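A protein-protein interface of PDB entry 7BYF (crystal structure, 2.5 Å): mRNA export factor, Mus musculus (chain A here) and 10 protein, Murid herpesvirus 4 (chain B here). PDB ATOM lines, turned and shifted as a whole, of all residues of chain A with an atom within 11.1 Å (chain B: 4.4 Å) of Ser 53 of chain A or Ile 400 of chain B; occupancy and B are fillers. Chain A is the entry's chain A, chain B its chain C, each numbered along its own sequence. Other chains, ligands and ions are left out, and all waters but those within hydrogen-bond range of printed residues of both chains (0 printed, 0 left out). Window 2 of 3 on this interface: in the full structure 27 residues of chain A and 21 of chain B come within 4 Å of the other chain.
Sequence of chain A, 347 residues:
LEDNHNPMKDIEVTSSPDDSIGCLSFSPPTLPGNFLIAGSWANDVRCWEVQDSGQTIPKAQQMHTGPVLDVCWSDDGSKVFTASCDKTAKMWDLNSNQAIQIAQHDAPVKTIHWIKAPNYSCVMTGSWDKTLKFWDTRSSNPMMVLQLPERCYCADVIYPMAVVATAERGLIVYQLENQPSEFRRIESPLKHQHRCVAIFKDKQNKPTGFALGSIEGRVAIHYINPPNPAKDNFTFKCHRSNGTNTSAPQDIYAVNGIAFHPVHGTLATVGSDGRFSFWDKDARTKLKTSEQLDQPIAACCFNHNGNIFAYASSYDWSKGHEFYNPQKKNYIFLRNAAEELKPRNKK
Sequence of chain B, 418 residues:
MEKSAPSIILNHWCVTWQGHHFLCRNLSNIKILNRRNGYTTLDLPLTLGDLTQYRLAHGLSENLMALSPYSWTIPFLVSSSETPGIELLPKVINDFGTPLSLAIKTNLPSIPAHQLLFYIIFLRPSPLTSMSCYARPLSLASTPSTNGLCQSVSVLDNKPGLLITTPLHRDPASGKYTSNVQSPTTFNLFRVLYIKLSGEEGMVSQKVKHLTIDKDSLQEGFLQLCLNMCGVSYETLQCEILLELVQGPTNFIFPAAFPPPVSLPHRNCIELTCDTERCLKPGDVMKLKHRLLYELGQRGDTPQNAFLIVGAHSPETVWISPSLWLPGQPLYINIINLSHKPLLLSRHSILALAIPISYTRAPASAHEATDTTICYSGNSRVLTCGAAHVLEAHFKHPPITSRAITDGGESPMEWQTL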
ATOM      1  N   LYS A   9      31.132  35.470  -7.341  1.00  0.00           N
ATOM      2  CA  LYS A   9      31.737  34.311  -6.626  1.00  0.00           C
ATOM      3  C   LYS A   9      30.962  33.026  -6.958  1.00  0.00           C
ATOM      4  O   LYS A   9      30.577  32.306  -6.015  1.00  0.00           O
ATOM      5  CB  LYS A   9      31.854  34.570  -5.118  1.00  0.00           C
ATOM      6  CG  LYS A   9      33.224  35.032  -4.641  1.00  0.00           C
ATOM      7  CD  LYS A   9      33.158  36.088  -3.558  1.00  0.00           C
ATOM      8  CE  LYS A   9      32.670  37.429  -4.066  1.00  0.00           C
ATOM      9  NZ  LYS A   9      32.707  38.464  -3.007  1.00  0.00           N
ATOM     10  N   ASP A  10      30.752  32.763  -8.253  1.00  0.00           N
ATOM     11  CA  ASP A  10      30.070  31.580  -8.738  1.00  0.00           C
ATOM     12  C   ASP A  10      31.060  30.436  -8.915  1.00  0.00           C
ATOM     13  O   ASP A  10      32.277  30.638  -8.945  1.00  0.00           O
ATOM     14  CB  ASP A  10      29.353  31.898 -10.045  1.00  0.00           C
ATOM     15  CG  ASP A  10      28.099  32.733  -9.819  1.00  0.00           C
ATOM     16  OD1 ASP A  10      27.457  32.540  -8.762  1.00  0.00           O
ATOM     17  OD2 ASP A  10      27.739  33.564 -10.688  1.00  0.00           O
ATOM     18  N   ILE A  11      30.518  29.217  -9.019  1.00  0.00           N
ATOM     19  CA  ILE A  11      31.360  28.056  -9.287  1.00  0.00           C
ATOM     20  C   ILE A  11      32.230  28.330 -10.499  1.00  0.00           C
ATOM     21  O   ILE A  11      31.770  28.867 -11.512  1.00  0.00           O
ATOM     22  CB  ILE A  11      30.526  26.787  -9.535  1.00  0.00           C
ATOM     23  CG1 ILE A  11      29.414  26.630  -8.492  1.00  0.00           C
ATOM     24  CG2 ILE A  11      31.446  25.568  -9.548  1.00  0.00           C
ATOM     25  CD1 ILE A  11      29.927  26.513  -7.115  1.00  0.00           C
ATOM     26  N   GLU A  12      33.506  27.946 -10.390  1.00  0.00           N
ATOM     27  CA  GLU A  12      34.491  28.138 -11.489  1.00  0.00           C
ATOM     28  C   GLU A  12      34.883  26.771 -12.060  1.00  0.00           C
ATOM     29  O   GLU A  12      35.467  25.963 -11.311  1.00  0.00           O
ATOM     30  CB  GLU A  12      35.720  28.892 -10.974  1.00  0.00           C
ATOM     31  CG  GLU A  12      36.956  28.686 -11.830  1.00  0.00           C
ATOM     32  CD  GLU A  12      38.146  29.544 -11.435  1.00  0.00           C
ATOM     33  OE1 GLU A  12      38.013  30.330 -10.476  1.00  0.00           O
ATOM     34  OE2 GLU A  12      39.203  29.424 -12.086  1.00  0.00           O
ATOM     35  N   THR A  14      36.915  23.885 -13.714  1.00  0.00           N
ATOM     36  CA  THR A  14      38.376  23.604 -13.726  1.00  0.00           C
ATOM     37  C   THR A  14      38.833  23.349 -15.167  1.00  0.00           C
ATOM     38  O   THR A  14      37.974  23.010 -16.006  1.00  0.00           O
ATOM     39  CB  THR A  14      38.719  22.422 -12.810  1.00  0.00           C
ATOM     40  OG1 THR A  14      38.331  21.219 -13.474  1.00  0.00           O
ATOM     41  CG2 THR A  14      38.038  22.505 -11.462  1.00  0.00           C
ATOM     42  N   GLY A  33      22.517  13.270 -15.418  1.00  0.00           N
ATOM     43  CA  GLY A  33      23.531  14.232 -15.017  1.00  0.00           C
ATOM     44  C   GLY A  33      23.633  15.389 -15.992  1.00  0.00           C
ATOM     45  O   GLY A  33      22.738  15.652 -16.800  1.00  0.00           O
ATOM     46  N   ASN A  34      24.744  16.102 -15.905  1.00  0.00           N
ATOM     47  CA  ASN A  34      24.930  17.251 -16.774  1.00  0.00           C
ATOM     48  C   ASN A  34      26.350  17.269 -17.327  1.00  0.00           C
ATOM     49  O   ASN A  34      27.322  17.062 -16.587  1.00  0.00           O
ATOM     50  CB  ASN A  34      24.613  18.548 -16.030  1.00  0.00           C
ATOM     51  CG  ASN A  34      23.131  18.696 -15.706  1.00  0.00           C
ATOM     52  OD1 ASN A  34      22.324  19.046 -16.569  1.00  0.00           O
ATOM     53  ND2 ASN A  34      22.772  18.452 -14.438  1.00  0.00           N
ATOM     54  N   GLU A  49      32.121  17.125 -16.970  1.00  0.00           N
ATOM     55  CA  GLU A  49      30.885  16.651 -16.328  1.00  0.00           C
ATOM     56  C   GLU A  49      30.576  17.625 -15.205  1.00  0.00           C
ATOM     57  O   GLU A  49      31.483  18.055 -14.600  1.00  0.00           O
ATOM     58  CB  GLU A  49      31.048  15.250 -15.780  1.00  0.00           C
ATOM     59  CG  GLU A  49      29.725  14.701 -15.334  1.00  0.00           C
ATOM     60  CD  GLU A  49      29.853  13.618 -14.299  1.00  0.00           C
ATOM     61  OE1 GLU A  49      30.952  13.089 -14.161  1.00  0.00           O
ATOM     62  OE2 GLU A  49      28.867  13.329 -13.645  1.00  0.00           O
ATOM     63  N   VAL A  50      29.322  18.001 -15.026  1.00  0.00           N
ATOM     64  CA  VAL A  50      28.976  18.908 -13.908  1.00  0.00           C
ATOM     65  C   VAL A  50      28.164  18.118 -12.890  1.00  0.00           C
ATOM     66  O   VAL A  50      27.124  17.643 -13.228  1.00  0.00           O
ATOM     67  CB  VAL A  50      28.210  20.153 -14.367  1.00  0.00           C
ATOM     68  CG1 VAL A  50      28.054  21.162 -13.266  1.00  0.00           C
ATOM     69  CG2 VAL A  50      28.834  20.802 -15.569  1.00  0.00           C
ATOM     70  N   GLN A  51      28.647  17.991 -11.667  1.00  0.00           N
ATOM     71  CA  GLN A  51      27.821  17.312 -10.652  1.00  0.00           C
ATOM     72  C   GLN A  51      26.827  18.304 -10.084  1.00  0.00           C
ATOM     73  O   GLN A  51      27.058  19.468 -10.186  1.00  0.00           O
ATOM     74  CB  GLN A  51      28.652  16.931  -9.447  1.00  0.00           C
ATOM     75  CG  GLN A  51      30.063  16.559  -9.781  1.00  0.00           C
ATOM     76  CD  GLN A  51      30.164  15.073  -9.935  1.00  0.00           C
ATOM     77  OE1 GLN A  51      29.285  14.433 -10.471  1.00  0.00           O
ATOM     78  NE2 GLN A  51      31.248  14.521  -9.449  1.00  0.00           N
ATOM     79  N   ASP A  52      25.842  17.805  -9.341  1.00  0.00           N
ATOM     80  CA  ASP A  52      24.819  18.626  -8.644  1.00  0.00           C
ATOM     81  C   ASP A  52      25.451  19.348  -7.446  1.00  0.00           C
ATOM     82  O   ASP A  52      24.967  20.376  -7.043  1.00  0.00           O
ATOM     83  CB  ASP A  52      23.632  17.770  -8.234  1.00  0.00           C
ATOM     84  CG  ASP A  52      22.945  17.021  -9.352  1.00  0.00           C
ATOM     85  OD1 ASP A  52      23.282  17.239 -10.505  1.00  0.00           O
ATOM     86  OD2 ASP A  52      22.080  16.231  -9.050  1.00  0.00           O
ATOM     87  N   SER A  53      26.571  18.832  -6.950  1.00  0.00           N
ATOM     88  CA  SER A  53      27.377  19.416  -5.866  1.00  0.00           C
ATOM     89  C   SER A  53      28.061  20.690  -6.342  1.00  0.00           C
ATOM     90  O   SER A  53      28.372  21.497  -5.515  1.00  0.00           O
ATOM     91  CB  SER A  53      28.360  18.433  -5.384  1.00  0.00           C
ATOM     92  OG  SER A  53      29.601  18.573  -6.016  1.00  0.00           O
ATOM     93  N   GLY A  54      28.265  20.845  -7.638  1.00  0.00           N
ATOM     94  CA  GLY A  54      28.890  22.048  -8.179  1.00  0.00           C
ATOM     95  C   GLY A  54      30.280  21.748  -8.670  1.00  0.00           C
ATOM     96  O   GLY A  54      30.917  22.637  -9.162  1.00  0.00           O
ATOM     97  N   GLN A  55      30.689  20.497  -8.572  1.00  0.00           N
ATOM     98  CA  GLN A  55      32.034  20.140  -9.013  1.00  0.00           C
ATOM     99  C   GLN A  55      32.005  19.819 -10.497  1.00  0.00           C
ATOM    100  O   GLN A  55      30.963  19.470 -11.018  1.00  0.00           O
ATOM    101  CB  GLN A  55      32.581  19.002  -8.173  1.00  0.00           C
ATOM    102  CG  GLN A  55      34.037  19.210  -7.858  1.00  0.00           C
ATOM    103  CD  GLN A  55      34.523  18.086  -7.000  1.00  0.00           C
ATOM    104  OE1 GLN A  55      35.557  17.491  -7.276  1.00  0.00           O
ATOM    105  NE2 GLN A  55      33.770  17.796  -5.950  1.00  0.00           N
ATOM    106  N   THR A  56      33.153  19.969 -11.126  1.00  0.00           N
ATOM    107  CA  THR A  56      33.244  19.785 -12.574  1.00  0.00           C
ATOM    108  C   THR A  56      34.418  18.879 -12.849  1.00  0.00           C
ATOM    109  O   THR A  56      35.404  19.102 -12.259  1.00  0.00           O
ATOM    110  CB  THR A  56      33.339  21.128 -13.289  1.00  0.00           C
ATOM    111  OG1 THR A  56      34.467  21.807 -12.772  1.00  0.00           O
ATOM    112  CG2 THR A  56      32.124  21.994 -13.099  1.00  0.00           C
ATOM    113  N   ILE A  57      34.262  17.879 -13.696  1.00  0.00           N
ATOM    114  CA  ILE A  57      35.406  16.976 -13.961  1.00  0.00           C
ATOM    115  C   ILE A  57      35.733  16.998 -15.443  1.00  0.00           C
ATOM    116  O   ILE A  57      34.903  16.601 -16.204  1.00  0.00           O
ATOM    117  CB  ILE A  57      35.097  15.546 -13.490  1.00  0.00           C
ATOM    118  CG1 ILE A  57      34.899  15.460 -11.981  1.00  0.00           C
ATOM    119  CG2 ILE A  57      36.177  14.599 -13.944  1.00  0.00           C
ATOM    120  CD1 ILE A  57      33.475  15.559 -11.572  1.00  0.00           C
ATOM    121  N   ASN A 303      21.157  24.593 -18.470  1.00  0.00           N
ATOM    122  CA  ASN A 303      21.118  23.144 -18.640  1.00  0.00           C
ATOM    123  C   ASN A 303      19.680  22.698 -18.900  1.00  0.00           C
ATOM    124  O   ASN A 303      18.763  23.519 -18.987  1.00  0.00           O
ATOM    125  CB  ASN A 303      21.734  22.423 -17.441  1.00  0.00           C
ATOM    126  CG  ASN A 303      20.832  22.408 -16.236  1.00  0.00           C
ATOM    127  OD1 ASN A 303      20.161  23.399 -15.924  1.00  0.00           O
ATOM    128  ND2 ASN A 303      20.803  21.269 -15.548  1.00  0.00           N
ATOM    129  N   ASN A 307      18.483  24.443 -13.856  1.00  0.00           N
ATOM    130  CA  ASN A 307      19.140  24.551 -12.572  1.00  0.00           C
ATOM    131  C   ASN A 307      20.489  25.240 -12.697  1.00  0.00           C
ATOM    132  O   ASN A 307      20.964  25.858 -11.735  1.00  0.00           O
ATOM    133  CB  ASN A 307      19.306  23.153 -11.972  1.00  0.00           C
ATOM    134  CG  ASN A 307      17.996  22.579 -11.438  1.00  0.00           C
ATOM    135  OD1 ASN A 307      16.929  23.195 -11.564  1.00  0.00           O
ATOM    136  ND2 ASN A 307      18.074  21.386 -10.855  1.00  0.00           N
ATOM    137  N   ILE A 308      21.127  25.146 -13.865  1.00  0.00           N
ATOM    138  CA  ILE A 308      22.471  25.675 -14.044  1.00  0.00           C
ATOM    139  C   ILE A 308      22.443  26.764 -15.109  1.00  0.00           C
ATOM    140  O   ILE A 308      21.843  26.588 -16.170  1.00  0.00           O
ATOM    141  CB  ILE A 308      23.467  24.560 -14.398  1.00  0.00           C
ATOM    142  CG1 ILE A 308      23.202  23.336 -13.531  1.00  0.00           C
ATOM    143  CG2 ILE A 308      24.878  25.014 -14.091  1.00  0.00           C
ATOM    144  CD1 ILE A 308      24.270  22.271 -13.634  1.00  0.00           C
ATOM    145  N   LEU A 334      29.549  28.674 -13.320  1.00  0.00           N
ATOM    146  CA  LEU A 334      28.270  28.004 -13.116  1.00  0.00           C
ATOM    147  C   LEU A 334      27.544  28.644 -11.945  1.00  0.00           C
ATOM    148  O   LEU A 334      28.148  28.934 -10.908  1.00  0.00           O
ATOM    149  CB  LEU A 334      28.464  26.530 -12.821  1.00  0.00           C
ATOM    150  CG  LEU A 334      29.466  25.896 -13.767  1.00  0.00           C
ATOM    151  CD1 LEU A 334      29.722  24.483 -13.291  1.00  0.00           C
ATOM    152  CD2 LEU A 334      28.942  25.941 -15.213  1.00  0.00           C
ATOM    153  N   ARG A 335      26.266  28.963 -12.162  1.00  0.00           N
ATOM    154  CA  ARG A 335      25.454  29.642 -11.119  1.00  0.00           C
ATOM    155  C   ARG A 335      24.101  28.942 -10.985  1.00  0.00           C
ATOM    156  O   ARG A 335      23.487  28.620 -12.022  1.00  0.00           O
ATOM    157  CB  ARG A 335      25.272  31.123 -11.466  1.00  0.00           C
ATOM    158  CG  ARG A 335      24.086  31.784 -10.776  1.00  0.00           C
ATOM    159  CD  ARG A 335      24.206  33.295 -10.739  1.00  0.00           C
ATOM    160  NE  ARG A 335      24.879  33.769  -9.537  1.00  0.00           N
ATOM    161  CZ  ARG A 335      24.563  34.884  -8.888  1.00  0.00           C
ATOM    162  NH1 ARG A 335      25.234  35.231  -7.804  1.00  0.00           N
ATOM    163  NH2 ARG A 335      23.578  35.647  -9.326  1.00  0.00           N
ATOM    164  N   ASN A 336      23.670  28.723  -9.741  1.00  0.00           N
ATOM    165  CA  ASN A 336      22.395  28.074  -9.451  1.00  0.00           C
ATOM    166  C   ASN A 336      21.226  28.993  -9.801  1.00  0.00           C
ATOM    167  O   ASN A 336      21.030  30.029  -9.158  1.00  0.00           O
ATOM    168  CB  ASN A 336      22.340  27.693  -7.978  1.00  0.00           C
ATOM    169  CG  ASN A 336      21.305  26.635  -7.691  1.00  0.00           C
ATOM    170  OD1 ASN A 336      20.102  26.828  -7.910  1.00  0.00           O
ATOM    171  ND2 ASN A 336      21.768  25.510  -7.168  1.00  0.00           N
ATOM    172  N   TRP B  17      25.345  28.087   6.636  1.00  0.00           N
ATOM    173  CA  TRP B  17      25.564  26.687   6.180  1.00  0.00           C
ATOM    174  C   TRP B  17      27.036  26.303   6.368  1.00  0.00           C
ATOM    175  O   TRP B  17      27.882  26.814   5.607  1.00  0.00           O
ATOM    176  CB  TRP B  17      25.117  26.520   4.722  1.00  0.00           C
ATOM    177  CG  TRP B  17      25.321  25.137   4.182  1.00  0.00           C
ATOM    178  CD1 TRP B  17      26.262  24.737   3.277  1.00  0.00           C
ATOM    179  CD2 TRP B  17      24.560  23.961   4.513  1.00  0.00           C
ATOM    180  NE1 TRP B  17      26.140  23.397   3.024  1.00  0.00           N
ATOM    181  CE2 TRP B  17      25.104  22.894   3.767  1.00  0.00           C
ATOM    182  CE3 TRP B  17      23.478  23.706   5.362  1.00  0.00           C
ATOM    183  CZ2 TRP B  17      24.600  21.597   3.849  1.00  0.00           C
ATOM    184  CZ3 TRP B  17      22.980  22.424   5.442  1.00  0.00           C
ATOM    185  CH2 TRP B  17      23.536  21.386   4.694  1.00  0.00           C
ATOM    186  N   GLY B  19      28.278  23.356   5.840  1.00  0.00           N
ATOM    187  CA  GLY B  19      28.618  22.474   4.709  1.00  0.00           C
ATOM    188  C   GLY B  19      27.829  21.177   4.755  1.00  0.00           C
ATOM    189  O   GLY B  19      27.551  20.615   3.677  1.00  0.00           O
ATOM    190  N   HIS B  58      21.955  25.586  -2.820  1.00  0.00           N
ATOM    191  CA  HIS B  58      22.862  24.503  -2.401  1.00  0.00           C
ATOM    192  C   HIS B  58      23.340  23.829  -3.646  1.00  0.00           C
ATOM    193  O   HIS B  58      22.533  23.495  -4.414  1.00  0.00           O
ATOM    194  CB  HIS B  58      22.112  23.539  -1.510  1.00  0.00           C
ATOM    195  CG  HIS B  58      21.693  24.211  -0.278  1.00  0.00           C
ATOM    196  ND1 HIS B  58      22.488  24.283   0.802  1.00  0.00           N
ATOM    197  CD2 HIS B  58      20.593  24.894   0.010  1.00  0.00           C
ATOM    198  CE1 HIS B  58      21.892  24.974   1.706  1.00  0.00           C
ATOM    199  NE2 HIS B  58      20.749  25.344   1.244  1.00  0.00           N
ATOM    200  N   GLY B  59      24.648  23.770  -3.843  1.00  0.00           N
ATOM    201  CA  GLY B  59      25.280  23.301  -5.062  1.00  0.00           C
ATOM    202  C   GLY B  59      24.599  23.834  -6.306  1.00  0.00           C
ATOM    203  O   GLY B  59      24.255  25.026  -6.376  1.00  0.00           O
ATOM    204  N   LEU B  67      19.865  16.762  -3.414  1.00  0.00           N
ATOM    205  CA  LEU B  67      21.268  16.288  -3.559  1.00  0.00           C
ATOM    206  C   LEU B  67      21.303  14.766  -3.376  1.00  0.00           C
ATOM    207  O   LEU B  67      20.443  14.245  -2.644  1.00  0.00           O
ATOM    208  CB  LEU B  67      22.140  16.989  -2.513  1.00  0.00           C
ATOM    209  CG  LEU B  67      22.591  18.402  -2.873  1.00  0.00           C
ATOM    210  CD1 LEU B  67      23.826  18.797  -2.078  1.00  0.00           C
ATOM    211  CD2 LEU B  67      22.860  18.521  -4.366  1.00  0.00           C
ATOM    212  N   TYR B  70      21.695  13.982   0.258  1.00  0.00           N
ATOM    213  CA  TYR B  70      20.731  14.590   1.215  1.00  0.00           C
ATOM    214  C   TYR B  70      19.333  14.060   0.897  1.00  0.00           C
ATOM    215  O   TYR B  70      18.491  14.228   1.748  1.00  0.00           O
ATOM    216  CB  TYR B  70      20.906  16.103   1.351  1.00  0.00           C
ATOM    217  CG  TYR B  70      22.223  16.538   1.923  1.00  0.00           C
ATOM    218  CD1 TYR B  70      23.344  16.643   1.137  1.00  0.00           C
ATOM    219  CD2 TYR B  70      22.348  16.865   3.254  1.00  0.00           C
ATOM    220  CE1 TYR B  70      24.561  17.006   1.669  1.00  0.00           C
ATOM    221  CE2 TYR B  70      23.553  17.252   3.796  1.00  0.00           C
ATOM    222  CZ  TYR B  70      24.669  17.331   2.999  1.00  0.00           C
ATOM    223  OH  TYR B  70      25.863  17.707   3.510  1.00  0.00           O
ATOM    224  N   PRO B 398      28.877  14.870   2.455  1.00  0.00           N
ATOM    225  CA  PRO B 398      29.939  15.644   1.802  1.00  0.00           C
ATOM    226  C   PRO B 398      29.651  17.151   1.862  1.00  0.00           C
ATOM    227  O   PRO B 398      28.492  17.524   1.869  1.00  0.00           O
ATOM    228  CB  PRO B 398      29.893  15.151   0.349  1.00  0.00           C
ATOM    229  CG  PRO B 398      28.459  14.710   0.156  1.00  0.00           C
ATOM    230  CD  PRO B 398      28.047  14.138   1.497  1.00  0.00           C
ATOM    231  N   PRO B 399      30.684  18.022   1.905  1.00  0.00           N
ATOM    232  CA  PRO B 399      30.476  19.473   1.965  1.00  0.00           C
ATOM    233  C   PRO B 399      29.997  20.031   0.617  1.00  0.00           C
ATOM    234  O   PRO B 399      30.677  19.830  -0.373  1.00  0.00           O
ATOM    235  CB  PRO B 399      31.874  20.014   2.295  1.00  0.00           C
ATOM    236  CG  PRO B 399      32.813  18.986   1.704  1.00  0.00           C
ATOM    237  CD  PRO B 399      32.104  17.660   1.894  1.00  0.00           C
ATOM    238  N   ILE B 400      28.847  20.712   0.620  1.00  0.00           N
ATOM    239  CA  ILE B 400      28.272  21.306  -0.625  1.00  0.00           C
ATOM    240  C   ILE B 400      28.351  22.833  -0.523  1.00  0.00           C
ATOM    241  O   ILE B 400      27.776  23.392   0.433  1.00  0.00           O
ATOM    242  CB  ILE B 400      26.825  20.822  -0.846  1.00  0.00           C
ATOM    243  CG1 ILE B 400      26.694  19.311  -0.640  1.00  0.00           C
ATOM    244  CG2 ILE B 400      26.316  21.251  -2.213  1.00  0.00           C
ATOM    245  CD1 ILE B 400      27.005  18.494  -1.873  1.00  0.00           C
ATOM    246  N   THR B 401      29.038  23.473  -1.475  1.00  0.00           N
ATOM    247  CA  THR B 401      29.184  24.954  -1.484  1.00  0.00           C
ATOM    248  C   THR B 401      27.868  25.591  -1.947  1.00  0.00           C
ATOM    249  O   THR B 401      27.558  25.497  -3.151  1.00  0.00           O
ATOM    250  CB  THR B 401      30.361  25.387  -2.368  1.00  0.00           C
ATOM    251  OG1 THR B 401      31.534  24.720  -1.902  1.00  0.00           O
ATOM    252  CG2 THR B 401      30.584  26.884  -2.356  1.00  0.00           C
ATOM    253  N   SER B 402      27.133  26.212  -1.017  1.00  0.00           N
ATOM    254  CA  SER B 402      25.838  26.867  -1.343  1.00  0.00           C
ATOM    255  C   SER B 402      25.979  28.388  -1.215  1.00  0.00           C
ATOM    256  O   SER B 402      26.844  28.839  -0.438  1.00  0.00           O
ATOM    257  CB  SER B 402      24.732  26.342  -0.465  1.00  0.00           C
ATOM    258  OG  SER B 402      24.980  24.994  -0.091  1.00  0.00           O
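ND2 of Asn 336 of chain A lies within hydrogen-bond range of O of His 58 of chain B (3.5 Å). The backbone carbonyl oxygen (O) of Gly 59 of chain B is in hydrogen-bond range of the side-chain amide nitrogen (ND2) of Asn 336 of chain A.
The side-chain hydroxyl (OG) of Ser 53 of chain A lies within hydrogen-bond range of the backbone NH (N) of Gln 55 of chain A (3.4 Å). NE1 of Trp 17 of chain B lies within hydrogen-bond range of O of Ile 400 of chain B (3.1 Å). N of Ile 400 of chain B lies within hydrogen-bond range of O of Gly 19 of chain B, at 3.3 Å. A ring nitrogen (ND1) of His 58 of chain B sits at hydrogen-bond distance from the side-chain hydroxyl (OG) of Ser 402 of chain B (2.7 Å). The backbone carbonyl oxygen (O) of Thr 401 of chain B is in hydrogen-bond range of the backbone NH (N) of Gly 59 of chain B (3.5 Å). The backbone carbonyl oxygen of Ile 400 of chain B lies within hydrogen-bond range of the side-chain hydroxyl of Ser 402 of chain B (3.3 Å).
Among the printed residues, merely in contact across the chains: Asp 52 of chain A with Gly 59 of chain B (3.5 Å), Ser 53 of chain A with Gly 59 of chain B (3.6 Å), Ser 53 of chain A with Ile 400 of chain B (3.8 Å) and Asp 52 of chain A with Leu 67 of chain B (3.9 Å).
Of the printed residues of chain B, Asp 52 of chain A touches Gly 59 (3.5 Å) and Leu 67 (3.9 Å). Ser 53 of chain A touches just these residues of chain B: Gly 59 (3.6 Å) and Ile 400 (3.8 Å). Asn 303 of chain A touches none of the printed residues of chain B. Printed residues of chain B within 4 Å of Asn 336 of chain A: His 58 and Gly 59. No residue of chain A comes within 4 Å of Gly 19 of chain B. Of the printed residues of chain A, His 58 of chain B touches Asn 336 (3.5 Å). Gly 59 of chain B touches three residues of chain A. Of the printed residues of chain A, Leu 67 of chain B touches Asp 52. No residue of chain A comes within 4 Å of Pro 398 of chain B. No residue of chain A comes within 4 Å of Pro 399 of chain B. Ser 402 of chain B touches none of the printed residues of chain A. The nearest printed residue of chain B that does not touch Ser 53 of chain A is Leu 67 of chain B (4.5 Å). The nearest residue of chain A that does not touch Ile 400 of chain B is Asp 52 of chain A (5.1 Å). The nearest printed residue of chain A that does not touch His 58 of chain B is Asp 52 of chain A (4.8 Å).
Of the 11 printed residues of chain B, 4 touch a printed residue of chain A. Hydrophobic or aromatic side chains of chain B within 4 Å of the printed part of chain A: Leu 67 and Ile 400. Among the printed residues, no Asp or Glu carboxylate lies within 4 Å of a Lys or Arg side-chain nitrogen of the other chain.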
